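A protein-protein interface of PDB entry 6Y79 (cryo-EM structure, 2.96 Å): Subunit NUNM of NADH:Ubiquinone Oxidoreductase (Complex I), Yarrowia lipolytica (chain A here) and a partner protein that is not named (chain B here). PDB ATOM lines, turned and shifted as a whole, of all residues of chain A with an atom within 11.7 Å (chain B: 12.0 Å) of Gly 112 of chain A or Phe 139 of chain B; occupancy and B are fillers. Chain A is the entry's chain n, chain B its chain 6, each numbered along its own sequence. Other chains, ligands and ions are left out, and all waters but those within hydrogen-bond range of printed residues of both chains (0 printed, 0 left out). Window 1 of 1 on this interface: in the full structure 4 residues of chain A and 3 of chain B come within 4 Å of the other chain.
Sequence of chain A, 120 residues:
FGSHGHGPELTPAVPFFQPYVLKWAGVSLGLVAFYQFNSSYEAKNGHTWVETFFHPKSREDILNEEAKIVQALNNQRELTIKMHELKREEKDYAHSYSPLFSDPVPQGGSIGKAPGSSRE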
ATOM      1  N   GLN A 107      28.838  21.411  -5.913  1.00  0.00           N
ATOM      2  CA  GLN A 107      27.539  22.046  -5.582  1.00  0.00           C
ATOM      3  C   GLN A 107      26.406  21.033  -5.374  1.00  0.00           C
ATOM      4  O   GLN A 107      25.285  21.196  -5.857  1.00  0.00           O
ATOM      5  CB  GLN A 107      27.149  23.130  -6.602  1.00  0.00           C
ATOM      6  CG  GLN A 107      27.040  22.718  -8.037  1.00  0.00           C
ATOM      7  CD  GLN A 107      26.404  23.777  -8.873  1.00  0.00           C
ATOM      8  OE1 GLN A 107      26.635  24.974  -8.665  1.00  0.00           O
ATOM      9  NE2 GLN A 107      25.519  23.350  -9.787  1.00  0.00           N
ATOM     10  N   GLY A 108      26.696  19.988  -4.604  1.00  0.00           N
ATOM     11  CA  GLY A 108      25.824  18.831  -4.518  1.00  0.00           C
ATOM     12  C   GLY A 108      24.988  18.833  -3.253  1.00  0.00           C
ATOM     13  O   GLY A 108      25.435  19.286  -2.201  1.00  0.00           O
ATOM     14  N   GLY A 109      23.783  18.288  -3.365  1.00  0.00           N
ATOM     15  CA  GLY A 109      22.881  18.201  -2.232  1.00  0.00           C
ATOM     16  C   GLY A 109      21.866  19.325  -2.167  1.00  0.00           C
ATOM     17  O   GLY A 109      21.810  20.073  -1.188  1.00  0.00           O
ATOM     18  N   SER A 110      21.084  19.505  -3.226  1.00  0.00           N
ATOM     19  CA  SER A 110      20.268  20.707  -3.346  1.00  0.00           C
ATOM     20  C   SER A 110      18.786  20.481  -3.043  1.00  0.00           C
ATOM     21  O   SER A 110      17.942  20.610  -3.928  1.00  0.00           O
ATOM     22  CB  SER A 110      20.452  21.297  -4.731  1.00  0.00           C
ATOM     23  OG  SER A 110      19.679  22.469  -4.880  1.00  0.00           O
ATOM     24  N   ILE A 111      18.451  20.210  -1.762  1.00  0.00           N
ATOM     25  CA  ILE A 111      17.076  20.461  -1.317  1.00  0.00           C
ATOM     26  C   ILE A 111      17.057  21.278  -0.018  1.00  0.00           C
ATOM     27  O   ILE A 111      16.470  22.357   0.008  1.00  0.00           O
ATOM     28  CB  ILE A 111      16.188  19.185  -1.199  1.00  0.00           C
ATOM     29  CG1 ILE A 111      16.649  18.114  -0.207  1.00  0.00           C
ATOM     30  CG2 ILE A 111      15.944  18.494  -2.542  1.00  0.00           C
ATOM     31  CD1 ILE A 111      15.597  17.074  -0.001  1.00  0.00           C
ATOM     32  N   GLY A 112      17.691  20.827   1.060  1.00  0.00           N
ATOM     33  CA  GLY A 112      17.475  21.494   2.333  1.00  0.00           C
ATOM     34  C   GLY A 112      18.609  22.436   2.648  1.00  0.00           C
ATOM     35  O   GLY A 112      19.055  22.542   3.794  1.00  0.00           O
ATOM     36  N   LYS A 113      19.080  23.131   1.620  1.00  0.00           N
ATOM     37  CA  LYS A 113      20.399  23.731   1.666  1.00  0.00           C
ATOM     38  C   LYS A 113      20.369  25.057   2.410  1.00  0.00           C
ATOM     39  O   LYS A 113      19.369  25.779   2.402  1.00  0.00           O
ATOM     40  CB  LYS A 113      20.953  23.879   0.245  1.00  0.00           C
ATOM     41  CG  LYS A 113      20.922  25.254  -0.362  1.00  0.00           C
ATOM     42  CD  LYS A 113      21.387  25.204  -1.800  1.00  0.00           C
ATOM     43  CE  LYS A 113      21.469  26.596  -2.385  1.00  0.00           C
ATOM     44  NZ  LYS A 113      21.881  26.577  -3.809  1.00  0.00           N
ATOM     45  N   ALA A 114      21.449  25.331   3.093  1.00  0.00           N
ATOM     46  CA  ALA A 114      21.690  26.504   3.914  1.00  0.00           C
ATOM     47  C   ALA A 114      22.374  27.572   3.081  1.00  0.00           C
ATOM     48  O   ALA A 114      23.252  27.245   2.281  1.00  0.00           O
ATOM     49  CB  ALA A 114      22.563  26.143   5.106  1.00  0.00           C
ATOM     50  N   PRO A 115      21.967  28.834   3.165  1.00  0.00           N
ATOM     51  CA  PRO A 115      22.825  29.896   2.627  1.00  0.00           C
ATOM     52  C   PRO A 115      24.028  30.139   3.527  1.00  0.00           C
ATOM     53  O   PRO A 115      23.920  30.145   4.753  1.00  0.00           O
ATOM     54  CB  PRO A 115      21.890  31.106   2.560  1.00  0.00           C
ATOM     55  CG  PRO A 115      20.553  30.476   2.338  1.00  0.00           C
ATOM     56  CD  PRO A 115      20.563  29.273   3.234  1.00  0.00           C
ATOM     57  N   GLY A 116      25.187  30.329   2.899  1.00  0.00           N
ATOM     58  CA  GLY A 116      26.450  30.311   3.596  1.00  0.00           C
ATOM     59  C   GLY A 116      27.188  28.997   3.511  1.00  0.00           C
ATOM     60  O   GLY A 116      28.185  28.810   4.229  1.00  0.00           O
ATOM     61  N   SER A 117      26.735  28.083   2.654  1.00  0.00           N
ATOM     62  CA  SER A 117      27.270  26.736   2.599  1.00  0.00           C
ATOM     63  C   SER A 117      28.286  26.556   1.485  1.00  0.00           C
ATOM     64  O   SER A 117      28.740  25.434   1.244  1.00  0.00           O
ATOM     65  CB  SER A 117      26.134  25.741   2.435  1.00  0.00           C
ATOM     66  OG  SER A 117      25.487  25.986   1.193  1.00  0.00           O
ATOM     67  N   SER A 118      28.669  27.631   0.809  1.00  0.00           N
ATOM     68  CA  SER A 118      29.346  27.488  -0.480  1.00  0.00           C
ATOM     69  C   SER A 118      30.865  27.443  -0.335  1.00  0.00           C
ATOM     70  O   SER A 118      31.478  26.398  -0.573  1.00  0.00           O
ATOM     71  CB  SER A 118      28.894  28.613  -1.411  1.00  0.00           C
ATOM     72  OG  SER A 118      27.583  28.356  -1.876  1.00  0.00           O
ATOM     73  N   THR B 135      23.950  21.724  17.471  1.00  0.00           N
ATOM     74  CA  THR B 135      23.397  23.052  17.256  1.00  0.00           C
ATOM     75  C   THR B 135      22.118  22.910  16.439  1.00  0.00           C
ATOM     76  O   THR B 135      21.975  21.969  15.654  1.00  0.00           O
ATOM     77  CB  THR B 135      24.459  23.926  16.546  1.00  0.00           C
ATOM     78  OG1 THR B 135      25.505  24.243  17.472  1.00  0.00           O
ATOM     79  CG2 THR B 135      23.929  25.243  15.941  1.00  0.00           C
ATOM     80  N   GLN B 136      21.158  23.806  16.657  1.00  0.00           N
ATOM     81  CA  GLN B 136      19.985  23.875  15.800  1.00  0.00           C
ATOM     82  C   GLN B 136      20.155  24.956  14.755  1.00  0.00           C
ATOM     83  O   GLN B 136      20.461  26.105  15.079  1.00  0.00           O
ATOM     84  CB  GLN B 136      18.749  24.172  16.614  1.00  0.00           C
ATOM     85  CG  GLN B 136      18.573  23.161  17.630  1.00  0.00           C
ATOM     86  CD  GLN B 136      17.551  23.603  18.605  1.00  0.00           C
ATOM     87  OE1 GLN B 136      16.903  24.625  18.421  1.00  0.00           O
ATOM     88  NE2 GLN B 136      17.490  22.928  19.739  1.00  0.00           N
ATOM     89  N   ASP B 137      19.953  24.588  13.507  1.00  0.00           N
ATOM     90  CA  ASP B 137      19.815  25.549  12.433  1.00  0.00           C
ATOM     91  C   ASP B 137      18.478  25.310  11.753  1.00  0.00           C
ATOM     92  O   ASP B 137      18.054  24.163  11.591  1.00  0.00           O
ATOM     93  CB  ASP B 137      20.976  25.430  11.455  1.00  0.00           C
ATOM     94  CG  ASP B 137      21.108  24.047  10.892  1.00  0.00           C
ATOM     95  OD1 ASP B 137      21.393  23.116  11.671  1.00  0.00           O
ATOM     96  OD2 ASP B 137      20.926  23.885   9.672  1.00  0.00           O
ATOM     97  N   TRP B 138      17.808  26.396  11.382  1.00  0.00           N
ATOM     98  CA  TRP B 138      16.439  26.368  10.874  1.00  0.00           C
ATOM     99  C   TRP B 138      16.393  26.422   9.357  1.00  0.00           C
ATOM    100  O   TRP B 138      15.535  27.095   8.797  1.00  0.00           O
ATOM    101  CB  TRP B 138      15.633  27.525  11.460  1.00  0.00           C
ATOM    102  CG  TRP B 138      15.428  27.488  12.943  1.00  0.00           C
ATOM    103  CD1 TRP B 138      16.245  28.013  13.886  1.00  0.00           C
ATOM    104  CD2 TRP B 138      14.311  26.929  13.645  1.00  0.00           C
ATOM    105  NE1 TRP B 138      15.724  27.800  15.135  1.00  0.00           N
ATOM    106  CE2 TRP B 138      14.536  27.136  15.013  1.00  0.00           C
ATOM    107  CE3 TRP B 138      13.151  26.261  13.249  1.00  0.00           C
ATOM    108  CZ2 TRP B 138      13.649  26.705  15.986  1.00  0.00           C
ATOM    109  CZ3 TRP B 138      12.274  25.836  14.213  1.00  0.00           C
ATOM    110  CH2 TRP B 138      12.521  26.066  15.564  1.00  0.00           C
ATOM    111  N   PHE B 139      17.311  25.761   8.658  1.00  0.00           N
ATOM    112  CA  PHE B 139      17.402  25.905   7.209  1.00  0.00           C
ATOM    113  C   PHE B 139      16.564  24.902   6.428  1.00  0.00           C
ATOM    114  O   PHE B 139      16.434  25.057   5.212  1.00  0.00           O
ATOM    115  CB  PHE B 139      18.853  25.773   6.744  1.00  0.00           C
ATOM    116  CG  PHE B 139      19.742  26.894   7.178  1.00  0.00           C
ATOM    117  CD1 PHE B 139      19.645  28.144   6.595  1.00  0.00           C
ATOM    118  CD2 PHE B 139      20.708  26.683   8.144  1.00  0.00           C
ATOM    119  CE1 PHE B 139      20.482  29.167   6.989  1.00  0.00           C
ATOM    120  CE2 PHE B 139      21.545  27.697   8.541  1.00  0.00           C
ATOM    121  CZ  PHE B 139      21.435  28.939   7.959  1.00  0.00           C
ATOM    122  N   ASN B 140      16.002  23.885   7.073  1.00  0.00           N
ATOM    123  CA  ASN B 140      15.300  22.806   6.385  1.00  0.00           C
ATOM    124  C   ASN B 140      13.809  22.870   6.683  1.00  0.00           C
ATOM    125  O   ASN B 140      13.406  22.823   7.845  1.00  0.00           O
ATOM    126  CB  ASN B 140      15.853  21.447   6.809  1.00  0.00           C
ATOM    127  CG  ASN B 140      15.291  20.310   5.992  1.00  0.00           C
ATOM    128  OD1 ASN B 140      14.772  20.510   4.894  1.00  0.00           O
ATOM    129  ND2 ASN B 140      15.377  19.103   6.530  1.00  0.00           N
ATOM    130  N   ILE B 141      12.993  22.919   5.633  1.00  0.00           N
ATOM    131  CA  ILE B 141      11.581  23.257   5.754  1.00  0.00           C
ATOM    132  C   ILE B 141      10.656  22.063   5.624  1.00  0.00           C
ATOM    133  O   ILE B 141       9.435  22.243   5.722  1.00  0.00           O
ATOM    134  CB  ILE B 141      11.189  24.335   4.729  1.00  0.00           C
ATOM    135  CG1 ILE B 141      11.727  23.950   3.356  1.00  0.00           C
ATOM    136  CG2 ILE B 141      11.729  25.652   5.140  1.00  0.00           C
ATOM    137  CD1 ILE B 141      11.464  24.951   2.283  1.00  0.00           C
ATOM    138  N   GLU B 142      11.168  20.853   5.415  1.00  0.00           N
ATOM    139  CA  GLU B 142      10.249  19.757   5.144  1.00  0.00           C
ATOM    140  C   GLU B 142      10.765  18.438   5.693  1.00  0.00           C
ATOM    141  O   GLU B 142      11.933  18.303   6.060  1.00  0.00           O
ATOM    142  CB  GLU B 142       9.980  19.619   3.657  1.00  0.00           C
ATOM    143  CG  GLU B 142      11.214  19.572   2.821  1.00  0.00           C
ATOM    144  CD  GLU B 142      10.874  19.370   1.372  1.00  0.00           C
ATOM    145  OE1 GLU B 142       9.688  19.538   1.020  1.00  0.00           O
ATOM    146  OE2 GLU B 142      11.780  19.031   0.588  1.00  0.00           O
ATOM    147  N   ASN B 143       9.866  17.452   5.719  1.00  0.00           N
ATOM    148  CA  ASN B 143      10.124  16.166   6.361  1.00  0.00           C
ATOM    149  C   ASN B 143      10.825  15.224   5.386  1.00  0.00           C
ATOM    150  O   ASN B 143      10.353  14.135   5.055  1.00  0.00           O
ATOM    151  CB  ASN B 143       8.827  15.566   6.884  1.00  0.00           C
ATOM    152  CG  ASN B 143       9.042  14.667   8.087  1.00  0.00           C
ATOM    153  OD1 ASN B 143      10.124  14.635   8.671  1.00  0.00           O
ATOM    154  ND2 ASN B 143       8.001  13.937   8.468  1.00  0.00           N
ATOM    155  N   THR B 144      11.979  15.671   4.917  1.00  0.00           N
ATOM    156  CA  THR B 144      12.881  14.768   4.229  1.00  0.00           C
ATOM    157  C   THR B 144      13.636  13.998   5.295  1.00  0.00           C
ATOM    158  O   THR B 144      14.618  14.483   5.856  1.00  0.00           O
ATOM    159  CB  THR B 144      13.826  15.527   3.312  1.00  0.00           C
ATOM    160  OG1 THR B 144      13.067  16.351   2.424  1.00  0.00           O
ATOM    161  CG2 THR B 144      14.607  14.540   2.492  1.00  0.00           C
ATOM    162  N   THR B 145      13.154  12.807   5.607  1.00  0.00           N
ATOM    163  CA  THR B 145      13.922  11.926   6.460  1.00  0.00           C
ATOM    164  C   THR B 145      14.869  11.102   5.598  1.00  0.00           C
ATOM    165  O   THR B 145      15.040  11.346   4.403  1.00  0.00           O
ATOM    166  CB  THR B 145      13.004  11.043   7.299  1.00  0.00           C
ATOM    167  OG1 THR B 145      12.260  10.164   6.448  1.00  0.00           O
ATOM    168  CG2 THR B 145      12.052  11.898   8.103  1.00  0.00           C
ATOM    169  N   THR B 148      13.674   9.025   2.501  1.00  0.00           N
ATOM    170  CA  THR B 148      13.384   9.888   1.364  1.00  0.00           C
ATOM    171  C   THR B 148      14.641  10.212   0.569  1.00  0.00           C
ATOM    172  O   THR B 148      14.625  10.186  -0.666  1.00  0.00           O
ATOM    173  CB  THR B 148      12.715  11.169   1.852  1.00  0.00           C
ATOM    174  OG1 THR B 148      11.508  10.839   2.545  1.00  0.00           O
ATOM    175  CG2 THR B 148      12.384  12.074   0.684  1.00  0.00           C
ATOM    176  N   THR B 149      15.752  10.495   1.250  1.00  0.00           N
ATOM    177  CA  THR B 149      16.959  10.842   0.514  1.00  0.00           C
ATOM    178  C   THR B 149      17.602   9.606  -0.100  1.00  0.00           C
ATOM    179  O   THR B 149      18.204   9.699  -1.178  1.00  0.00           O
ATOM    180  CB  THR B 149      17.935  11.579   1.421  1.00  0.00           C
ATOM    181  OG1 THR B 149      17.212  12.549   2.177  1.00  0.00           O
ATOM    182  CG2 THR B 149      18.990  12.293   0.574  1.00  0.00           C
ATOM    183  N   ASN B 152      15.818   9.366  -3.157  1.00  0.00           N
ATOM    184  CA  ASN B 152      16.172  10.352  -4.172  1.00  0.00           C
ATOM    185  C   ASN B 152      17.459   9.980  -4.872  1.00  0.00           C
ATOM    186  O   ASN B 152      17.570  10.152  -6.085  1.00  0.00           O
ATOM    187  CB  ASN B 152      16.318  11.748  -3.551  1.00  0.00           C
ATOM    188  CG  ASN B 152      16.364  12.880  -4.583  1.00  0.00           C
ATOM    189  OD1 ASN B 152      16.230  12.664  -5.788  1.00  0.00           O
ATOM    190  ND2 ASN B 152      16.605  14.098  -4.105  1.00  0.00           N
ATOM    191  N   VAL B 153      18.413   9.409  -4.151  1.00  0.00           N
ATOM    192  CA  VAL B 153      19.729   9.218  -4.737  1.00  0.00           C
ATOM    193  C   VAL B 153      19.919   7.814  -5.316  1.00  0.00           C
ATOM    194  O   VAL B 153      20.689   7.641  -6.261  1.00  0.00           O
ATOM    195  CB  VAL B 153      20.769   9.597  -3.680  1.00  0.00           C
ATOM    196  CG1 VAL B 153      22.128   9.641  -4.261  1.00  0.00           C
ATOM    197  CG2 VAL B 153      20.447  10.983  -3.231  1.00  0.00           C
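The side-chain hydroxyl (OG) of Ser 117 of chain A sits at hydrogen-bond distance from the backbone carbonyl oxygen (O) of Ala 114 of chain A.
The side-chain carboxylate (OE2) of Glu 142 of chain B sits at hydrogen-bond distance from the side-chain hydroxyl (OG1) of Thr 144 of chain B.
CD1 of Ile 111 of chain A touches OG1 of Thr 144 of chain B, at 3.6 Å.
O of Gly 112 of chain A touches O of Phe 139 of chain B, 3.9 Å away.
Asn 140 of chain B touches Gly 112 of chain A.
CG of Phe 139 of chain B touches CB of Ala 114 of chain A, 3.6 Å away.
CD1 of Phe 139 of chain B touches CD of Pro 115 of chain A, at 3.7 Å.
Gly 112 of chain A touches just these residues of chain B: Phe 139 and Asn 140.
Phe 139 of chain B touches just these residues of chain A: Gly 112 (3.9 Å), Ala 114 (3.6 Å) and Pro 115 (3.7 Å).
No residue of chain B comes within 4 Å of Gly 109 of chain A.
No residue of chain B comes within 4 Å of Ser 110 of chain A.
Ile 111 of chain A touches one residue of chain B.
Of chain B, only Phe 139 comes within 4 Å of Pro 115 of chain A.
No residue of chain B comes within 4 Å of Gly 116 of chain A.
No residue of chain A comes within 4 Å of Ile 141 of chain B.
Printed residues of chain A within 4 Å of Thr 144 of chain B: Ile 111 (3.6 Å).
The nearest residue of chain A that does not touch Phe 139 of chain B is Lys 113 of chain A (4.1 Å).
Hydrophobic or aromatic side chains of chain B within 4 Å of the printed part of chain A: Phe 139.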
